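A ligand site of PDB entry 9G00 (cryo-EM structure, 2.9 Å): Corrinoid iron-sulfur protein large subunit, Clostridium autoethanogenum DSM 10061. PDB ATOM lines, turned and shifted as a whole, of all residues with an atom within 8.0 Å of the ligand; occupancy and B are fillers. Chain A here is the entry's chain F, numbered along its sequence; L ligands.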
ATOM      1  N   ILE A   8       1.182  19.131  20.188  1.00  0.00           N
ATOM      2  CA  ILE A   8       0.131  18.860  19.218  1.00  0.00           C
ATOM      3  C   ILE A   8      -0.822  20.033  19.069  1.00  0.00           C
ATOM      4  O   ILE A   8      -1.588  20.084  18.098  1.00  0.00           O
ATOM      5  CB  ILE A   8      -0.638  17.582  19.593  1.00  0.00           C
ATOM      6  CG1 ILE A   8      -1.618  17.848  20.743  1.00  0.00           C
ATOM      7  CG2 ILE A   8       0.322  16.455  19.944  1.00  0.00           C
ATOM      8  CD1 ILE A   8      -3.031  17.964  20.245  1.00  0.00           C
ATOM      9  N   PHE A   9      -0.809  20.984  20.008  1.00  0.00           N
ATOM     10  CA  PHE A   9      -1.641  22.177  19.863  1.00  0.00           C
ATOM     11  C   PHE A   9      -1.237  22.984  18.644  1.00  0.00           C
ATOM     12  O   PHE A   9      -2.076  23.671  18.049  1.00  0.00           O
ATOM     13  CB  PHE A   9      -1.565  23.046  21.113  1.00  0.00           C
ATOM     14  CG  PHE A   9      -2.553  24.172  21.138  1.00  0.00           C
ATOM     15  CD1 PHE A   9      -3.854  23.949  21.552  1.00  0.00           C
ATOM     16  CD2 PHE A   9      -2.184  25.447  20.763  1.00  0.00           C
ATOM     17  CE1 PHE A   9      -4.766  24.994  21.582  1.00  0.00           C
ATOM     18  CE2 PHE A   9      -3.093  26.480  20.787  1.00  0.00           C
ATOM     19  CZ  PHE A   9      -4.380  26.252  21.201  1.00  0.00           C
ATOM     20  N   THR A  12      -3.197  21.570  16.004  1.00  0.00           N
ATOM     21  CA  THR A  12      -4.626  21.749  16.182  1.00  0.00           C
ATOM     22  C   THR A  12      -5.113  22.976  15.412  1.00  0.00           C
ATOM     23  O   THR A  12      -4.403  23.982  15.357  1.00  0.00           O
ATOM     24  CB  THR A  12      -4.970  21.894  17.666  1.00  0.00           C
ATOM     25  OG1 THR A  12      -4.280  20.890  18.415  1.00  0.00           O
ATOM     26  CG2 THR A  12      -6.459  21.746  17.884  1.00  0.00           C
ATOM     27  N   PRO A  13      -6.293  22.920  14.789  1.00  0.00           N
ATOM     28  CA  PRO A  13      -6.797  24.105  14.079  1.00  0.00           C
ATOM     29  C   PRO A  13      -7.055  25.302  14.974  1.00  0.00           C
ATOM     30  O   PRO A  13      -7.133  26.421  14.461  1.00  0.00           O
ATOM     31  CB  PRO A  13      -8.093  23.587  13.430  1.00  0.00           C
ATOM     32  CG  PRO A  13      -8.469  22.369  14.205  1.00  0.00           C
ATOM     33  CD  PRO A  13      -7.178  21.757  14.617  1.00  0.00           C
ATOM     34  N   LYS A  14      -7.189  25.109  16.282  1.00  0.00           N
ATOM     35  CA  LYS A  14      -7.421  26.195  17.236  1.00  0.00           C
ATOM     36  C   LYS A  14      -8.705  26.950  16.898  1.00  0.00           C
ATOM     37  O   LYS A  14      -8.703  28.154  16.597  1.00  0.00           O
ATOM     38  CB  LYS A  14      -6.220  27.144  17.264  1.00  0.00           C
ATOM     39  CG  LYS A  14      -4.908  26.464  17.609  1.00  0.00           C
ATOM     40  CD  LYS A  14      -3.719  27.372  17.343  1.00  0.00           C
ATOM     41  CE  LYS A  14      -2.670  26.667  16.489  1.00  0.00           C
ATOM     42  NZ  LYS A  14      -3.212  26.211  15.185  1.00  0.00           N
ATOM     43  N   LYS A  15      -9.818  26.221  16.944  1.00  0.00           N
ATOM     44  CA  LYS A  15     -11.128  26.787  16.664  1.00  0.00           C
ATOM     45  C   LYS A  15     -12.040  26.832  17.887  1.00  0.00           C
ATOM     46  O   LYS A  15     -13.031  27.559  17.866  1.00  0.00           O
ATOM     47  CB  LYS A  15     -11.821  25.987  15.553  1.00  0.00           C
ATOM     48  CG  LYS A  15     -10.984  25.839  14.289  1.00  0.00           C
ATOM     49  CD  LYS A  15     -10.826  27.162  13.551  1.00  0.00           C
ATOM     50  CE  LYS A  15     -10.104  26.986  12.220  1.00  0.00           C
ATOM     51  NZ  LYS A  15      -8.631  26.818  12.367  1.00  0.00           N
ATOM     52  N   ASN A  16     -11.733  26.069  18.936  1.00  0.00           N
ATOM     53  CA  ASN A  16     -12.536  26.040  20.149  1.00  0.00           C
ATOM     54  C   ASN A  16     -14.015  25.778  19.823  1.00  0.00           C
ATOM     55  O   ASN A  16     -14.912  26.412  20.375  1.00  0.00           O
ATOM     56  CB  ASN A  16     -12.384  27.344  20.938  1.00  0.00           C
ATOM     57  CG  ASN A  16     -10.928  27.685  21.208  1.00  0.00           C
ATOM     58  OD1 ASN A  16     -10.038  26.862  21.047  1.00  0.00           O
ATOM     59  ND2 ASN A  16     -10.689  28.926  21.631  1.00  0.00           N
ATOM     60  N   CYS A  17     -14.250  24.836  18.915  1.00  0.00           N
ATOM     61  CA  CYS A  17     -15.588  24.520  18.442  1.00  0.00           C
ATOM     62  C   CYS A  17     -16.265  23.427  19.255  1.00  0.00           C
ATOM     63  O   CYS A  17     -17.446  23.137  19.019  1.00  0.00           O
ATOM     64  CB  CYS A  17     -15.551  24.115  16.970  1.00  0.00           C
ATOM     65  SG  CYS A  17     -14.475  22.744  16.586  1.00  0.00           S
ATOM     66  N   LYS A  18     -15.570  22.813  20.215  1.00  0.00           N
ATOM     67  CA  LYS A  18     -16.162  21.812  21.097  1.00  0.00           C
ATOM     68  C   LYS A  18     -16.646  20.570  20.344  1.00  0.00           C
ATOM     69  O   LYS A  18     -17.502  19.837  20.848  1.00  0.00           O
ATOM     70  CB  LYS A  18     -17.241  22.455  21.964  1.00  0.00           C
ATOM     71  CG  LYS A  18     -16.720  23.635  22.764  1.00  0.00           C
ATOM     72  CD  LYS A  18     -17.756  24.509  23.399  1.00  0.00           C
ATOM     73  CE  LYS A  18     -17.092  25.587  24.247  1.00  0.00           C
ATOM     74  NZ  LYS A  18     -18.081  26.408  24.964  1.00  0.00           N
ATOM     75  N   ASP A  19     -16.090  20.296  19.159  1.00  0.00           N
ATOM     76  CA  ASP A  19     -16.523  19.130  18.392  1.00  0.00           C
ATOM     77  C   ASP A  19     -15.988  17.842  19.031  1.00  0.00           C
ATOM     78  O   ASP A  19     -16.670  16.808  18.996  1.00  0.00           O
ATOM     79  CB  ASP A  19     -16.156  19.253  16.901  1.00  0.00           C
ATOM     80  CG  ASP A  19     -16.995  20.302  16.150  1.00  0.00           C
ATOM     81  OD1 ASP A  19     -17.705  21.099  16.793  1.00  0.00           O
ATOM     82  OD2 ASP A  19     -16.936  20.314  14.907  1.00  0.00           O
ATOM     83  N   CYS A  20     -14.799  17.885  19.670  1.00  0.00           N
ATOM     84  CA  CYS A  20     -14.185  16.708  20.321  1.00  0.00           C
ATOM     85  C   CYS A  20     -14.828  16.405  21.645  1.00  0.00           C
ATOM     86  O   CYS A  20     -14.425  15.435  22.298  1.00  0.00           O
ATOM     87  CB  CYS A  20     -12.695  16.883  20.668  1.00  0.00           C
ATOM     88  SG  CYS A  20     -12.282  18.461  21.409  1.00  0.00           S
ATOM     89  N   GLY A  21     -15.761  17.225  22.084  1.00  0.00           N
ATOM     90  CA  GLY A  21     -16.359  16.998  23.374  1.00  0.00           C
ATOM     91  C   GLY A  21     -15.680  17.741  24.497  1.00  0.00           C
ATOM     92  O   GLY A  21     -16.178  17.699  25.629  1.00  0.00           O
ATOM     93  N   PHE A  22     -14.544  18.401  24.243  1.00  0.00           N
ATOM     94  CA  PHE A  22     -13.879  19.203  25.241  1.00  0.00           C
ATOM     95  C   PHE A  22     -14.026  20.694  24.906  1.00  0.00           C
ATOM     96  O   PHE A  22     -14.108  21.063  23.736  1.00  0.00           O
ATOM     97  CB  PHE A  22     -12.389  18.853  25.338  1.00  0.00           C
ATOM     98  CG  PHE A  22     -12.113  17.561  26.053  1.00  0.00           C
ATOM     99  CD1 PHE A  22     -13.136  16.809  26.610  1.00  0.00           C
ATOM    100  CD2 PHE A  22     -10.817  17.094  26.191  1.00  0.00           C
ATOM    101  CE1 PHE A  22     -12.873  15.623  27.267  1.00  0.00           C
ATOM    102  CE2 PHE A  22     -10.551  15.918  26.847  1.00  0.00           C
ATOM    103  CZ  PHE A  22     -11.577  15.178  27.397  1.00  0.00           C
ATOM    104  N   PRO A  23     -14.060  21.563  25.937  1.00  0.00           N
ATOM    105  CA  PRO A  23     -14.355  22.984  25.653  1.00  0.00           C
ATOM    106  C   PRO A  23     -13.382  23.646  24.699  1.00  0.00           C
ATOM    107  O   PRO A  23     -13.795  24.205  23.682  1.00  0.00           O
ATOM    108  CB  PRO A  23     -14.306  23.619  27.049  1.00  0.00           C
ATOM    109  CG  PRO A  23     -14.608  22.506  27.993  1.00  0.00           C
ATOM    110  CD  PRO A  23     -13.967  21.297  27.376  1.00  0.00           C
ATOM    111  N   THR A  24     -12.078  23.596  24.995  1.00  0.00           N
ATOM    112  CA  THR A  24     -11.083  24.306  24.201  1.00  0.00           C
ATOM    113  C   THR A  24     -10.166  23.310  23.506  1.00  0.00           C
ATOM    114  O   THR A  24     -10.046  22.155  23.901  1.00  0.00           O
ATOM    115  CB  THR A  24     -10.261  25.262  25.063  1.00  0.00           C
ATOM    116  OG1 THR A  24      -9.481  24.509  26.005  1.00  0.00           O
ATOM    117  CG2 THR A  24     -11.164  26.236  25.809  1.00  0.00           C
ATOM    118  N   CYS A  25      -9.514  23.793  22.444  1.00  0.00           N
ATOM    119  CA  CYS A  25      -8.508  22.979  21.769  1.00  0.00           C
ATOM    120  C   CYS A  25      -7.362  22.647  22.715  1.00  0.00           C
ATOM    121  O   CYS A  25      -6.781  21.561  22.650  1.00  0.00           O
ATOM    122  CB  CYS A  25      -7.978  23.717  20.540  1.00  0.00           C
ATOM    123  SG  CYS A  25      -9.175  23.918  19.201  1.00  0.00           S
ATOM    124  N   LEU A  26      -7.007  23.585  23.593  1.00  0.00           N
ATOM    125  CA  LEU A  26      -5.970  23.307  24.585  1.00  0.00           C
ATOM    126  C   LEU A  26      -6.399  22.197  25.523  1.00  0.00           C
ATOM    127  O   LEU A  26      -5.600  21.311  25.865  1.00  0.00           O
ATOM    128  CB  LEU A  26      -5.628  24.573  25.367  1.00  0.00           C
ATOM    129  CG  LEU A  26      -4.440  24.460  26.316  1.00  0.00           C
ATOM    130  CD1 LEU A  26      -3.139  24.279  25.544  1.00  0.00           C
ATOM    131  CD2 LEU A  26      -4.374  25.678  27.219  1.00  0.00           C
ATOM    132  N   ALA A  27      -7.666  22.211  25.967  1.00  0.00           N
ATOM    133  CA  ALA A  27      -8.159  21.127  26.805  1.00  0.00           C
ATOM    134  C   ALA A  27      -8.075  19.793  26.065  1.00  0.00           C
ATOM    135  O   ALA A  27      -7.680  18.778  26.657  1.00  0.00           O
ATOM    136  CB  ALA A  27      -9.600  21.406  27.230  1.00  0.00           C
ATOM    137  N   PHE A  28      -8.429  19.784  24.787  1.00  0.00           N
ATOM    138  CA  PHE A  28      -8.221  18.599  23.955  1.00  0.00           C
ATOM    139  C   PHE A  28      -6.741  18.333  23.719  1.00  0.00           C
ATOM    140  O   PHE A  28      -6.367  17.189  23.456  1.00  0.00           O
ATOM    141  CB  PHE A  28      -8.951  18.777  22.618  1.00  0.00           C
ATOM    142  CG  PHE A  28      -8.793  17.614  21.686  1.00  0.00           C
ATOM    143  CD1 PHE A  28      -9.540  16.469  21.837  1.00  0.00           C
ATOM    144  CD2 PHE A  28      -7.877  17.668  20.639  1.00  0.00           C
ATOM    145  CE1 PHE A  28      -9.400  15.404  20.975  1.00  0.00           C
ATOM    146  CE2 PHE A  28      -7.727  16.609  19.770  1.00  0.00           C
ATOM    147  CZ  PHE A  28      -8.487  15.471  19.935  1.00  0.00           C
ATOM    148  N   SER A  29      -5.895  19.364  23.795  1.00  0.00           N
ATOM    149  CA  SER A  29      -4.482  19.180  23.491  1.00  0.00           C
ATOM    150  C   SER A  29      -3.757  18.428  24.596  1.00  0.00           C
ATOM    151  O   SER A  29      -2.996  17.493  24.318  1.00  0.00           O
ATOM    152  CB  SER A  29      -3.820  20.541  23.253  1.00  0.00           C
ATOM    153  OG  SER A  29      -2.446  20.374  22.976  1.00  0.00           O
ATOM    154  N   VAL A  32      -5.059  14.459  25.212  1.00  0.00           N
ATOM    155  CA  VAL A  32      -4.640  13.433  24.265  1.00  0.00           C
ATOM    156  C   VAL A  32      -3.172  13.070  24.477  1.00  0.00           C
ATOM    157  O   VAL A  32      -2.764  11.935  24.213  1.00  0.00           O
ATOM    158  CB  VAL A  32      -4.901  13.877  22.808  1.00  0.00           C
ATOM    159  CG1 VAL A  32      -6.380  14.193  22.621  1.00  0.00           C
ATOM    160  CG2 VAL A  32      -4.029  15.087  22.459  1.00  0.00           C
ATOM    161  N   ILE A  39      -7.127  10.734  19.543  1.00  0.00           N
ATOM    162  CA  ILE A  39      -7.135  11.738  18.485  1.00  0.00           C
ATOM    163  C   ILE A  39      -8.423  11.749  17.674  1.00  0.00           C
ATOM    164  O   ILE A  39      -8.692  12.753  16.988  1.00  0.00           O
ATOM    165  CB  ILE A  39      -5.920  11.543  17.553  1.00  0.00           C
ATOM    166  CG1 ILE A  39      -6.293  10.650  16.366  1.00  0.00           C
ATOM    167  CG2 ILE A  39      -4.751  10.941  18.320  1.00  0.00           C
ATOM    168  CD1 ILE A  39      -5.137  10.275  15.456  1.00  0.00           C
ATOM    169  N   GLY A  40      -9.214  10.687  17.720  1.00  0.00           N
ATOM    170  CA  GLY A  40     -10.338  10.565  16.803  1.00  0.00           C
ATOM    171  C   GLY A  40     -11.422  11.602  17.007  1.00  0.00           C
ATOM    172  O   GLY A  40     -12.158  11.901  16.058  1.00  0.00           O
ATOM    173  N   LYS A  41     -11.541  12.144  18.215  1.00  0.00           N
ATOM    174  CA  LYS A  41     -12.681  12.987  18.534  1.00  0.00           C
ATOM    175  C   LYS A  41     -12.712  14.266  17.710  1.00  0.00           C
ATOM    176  O   LYS A  41     -13.779  14.884  17.593  1.00  0.00           O
ATOM    177  CB  LYS A  41     -12.686  13.339  20.018  1.00  0.00           C
ATOM    178  CG  LYS A  41     -13.211  12.231  20.936  1.00  0.00           C
ATOM    179  CD  LYS A  41     -12.151  11.192  21.243  1.00  0.00           C
ATOM    180  CE  LYS A  41     -12.317   9.931  20.408  1.00  0.00           C
ATOM    181  NZ  LYS A  41     -11.256   8.934  20.698  1.00  0.00           N
ATOM    182  N   CYS A  42     -11.588  14.679  17.136  1.00  0.00           N
ATOM    183  CA  CYS A  42     -11.527  15.942  16.404  1.00  0.00           C
ATOM    184  C   CYS A  42     -11.685  15.682  14.916  1.00  0.00           C
ATOM    185  O   CYS A  42     -10.781  15.104  14.302  1.00  0.00           O
ATOM    186  CB  CYS A  42     -10.213  16.657  16.682  1.00  0.00           C
ATOM    187  SG  CYS A  42     -10.153  18.331  16.003  1.00  0.00           S
ATOM    188  N   PRO A  43     -12.808  16.087  14.291  1.00  0.00           N
ATOM    189  CA  PRO A  43     -12.959  15.849  12.843  1.00  0.00           C
ATOM    190  C   PRO A  43     -12.332  16.947  11.995  1.00  0.00           C
ATOM    191  O   PRO A  43     -12.008  16.718  10.831  1.00  0.00           O
ATOM    192  CB  PRO A  43     -14.486  15.808  12.650  1.00  0.00           C
ATOM    193  CG  PRO A  43     -15.091  15.935  14.039  1.00  0.00           C
ATOM    194  CD  PRO A  43     -14.053  16.595  14.873  1.00  0.00           C
ATOM    195  N   HIS A  44     -12.128  18.119  12.588  1.00  0.00           N
ATOM    196  CA  HIS A  44     -11.645  19.278  11.837  1.00  0.00           C
ATOM    197  C   HIS A  44     -10.135  19.259  11.624  1.00  0.00           C
ATOM    198  O   HIS A  44      -9.607  20.200  11.024  1.00  0.00           O
ATOM    199  CB  HIS A  44     -12.041  20.566  12.564  1.00  0.00           C
ATOM    200  CG  HIS A  44     -13.521  20.804  12.596  1.00  0.00           C
ATOM    201  ND1 HIS A  44     -14.425  19.983  11.958  1.00  0.00           N
ATOM    202  CD2 HIS A  44     -14.249  21.777  13.204  1.00  0.00           C
ATOM    203  CE1 HIS A  44     -15.652  20.442  12.160  1.00  0.00           C
ATOM    204  NE2 HIS A  44     -15.567  21.522  12.911  1.00  0.00           N
ATOM    205  N   MET A  45      -9.446  18.219  12.071  1.00  0.00           N
ATOM    206  CA  MET A  45      -8.014  18.131  11.844  1.00  0.00           C
ATOM    207  C   MET A  45      -7.702  18.062  10.355  1.00  0.00           C
ATOM    208  O   MET A  45      -8.350  17.339   9.599  1.00  0.00           O
ATOM    209  CB  MET A  45      -7.451  16.881  12.537  1.00  0.00           C
ATOM    210  CG  MET A  45      -7.278  17.019  14.049  1.00  0.00           C
ATOM    211  SD  MET A  45      -6.028  18.223  14.516  1.00  0.00           S
ATOM    212  CE  MET A  45      -4.565  17.541  13.725  1.00  0.00           C
HETATM  213 FE1  LIG L   1     -10.901  20.095  17.287  1.00  0.00          FE
HETATM  214 FE2  LIG L   1     -10.588  22.198  19.004  1.00  0.00          FE
HETATM  215 FE3  LIG L   1     -12.004  19.996  19.787  1.00  0.00          FE
HETATM  216 FE4  LIG L   1     -13.034  21.672  17.912  1.00  0.00          FE
HETATM  217  S1  LIG L   1     -12.600  22.177  20.086  1.00  0.00           S
HETATM  218  S2  LIG L   1     -12.997  19.396  17.835  1.00  0.00           S
HETATM  219  S3  LIG L   1     -11.144  22.303  16.798  1.00  0.00           S
HETATM  220  S4  LIG L   1      -9.790  20.077  19.272  1.00  0.00           S
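The backbone NH (N) of Cys 17 sits close to a sulfur (S1) of the ligand, at 3.3 Å. The side-chain sulfur of Cys 17 is bound to an iron atom (FE4) of the ligand (2.2 Å). An iron atom (FE2) of the ligand is bound by the side-chain sulfur of Cys 25 (2.2 Å). The backbone NH (N) of Cys 20 sits close to a sulfur (S2) of the ligand, at 3.0 Å. The side-chain sulfur (SG) of Cys 20 binds an iron atom (FE3) of the ligand, 2.3 Å away. The side-chain sulfur (SG) of Cys 42 binds an iron atom (FE1) of the ligand. A sulfur (S1) of the ligand lies close to the backbone NH of Lys 18 (3.0 Å). S2 of the ligand sits close to N of Asp 19 (3.5 Å).
SG of Cys 17 lies close to OD1 of Asp 19, 3.6 Å away. The side-chain amide oxygen (OD1) of Asn 16 sits at hydrogen-bond distance from the backbone NH (N) of Cys 25 (3.4 Å). The backbone NH (N) of Lys 15 lies close to the side-chain sulfur (SG) of Cys 25 (3.3 Å). N of Phe 22 sits close to SG of Cys 20 (3.6 Å). NE2 of His 44 sits at hydrogen-bond distance from OD2 of Asp 19 (2.7 Å). O of Pro 13 is in hydrogen-bond range of NZ of Lys 15, at 2.6 Å. O of Thr 12 is in hydrogen-bond range of NZ of Lys 14 (2.5 Å). OG1 of Thr 12 sits at hydrogen-bond distance from O of Ile 8, at 2.8 Å.
CG2 of Thr 12 touches S4 of the ligand, 3.98 Å away. Pro 13 touches the ligand (CG to S3, 3.7 Å). Lys 15 touches the ligand (CB to S3, 3.9 Å). Asn 16 touches the ligand. Phe 28 touches the ligand (CD2 to S4, 3.4 Å). Hydrophobic or aromatic side chains that line the ligand: Pro 13 and Phe 28. The nearest printed residue that does not touch the ligand is Phe 22 (4.1 Å).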
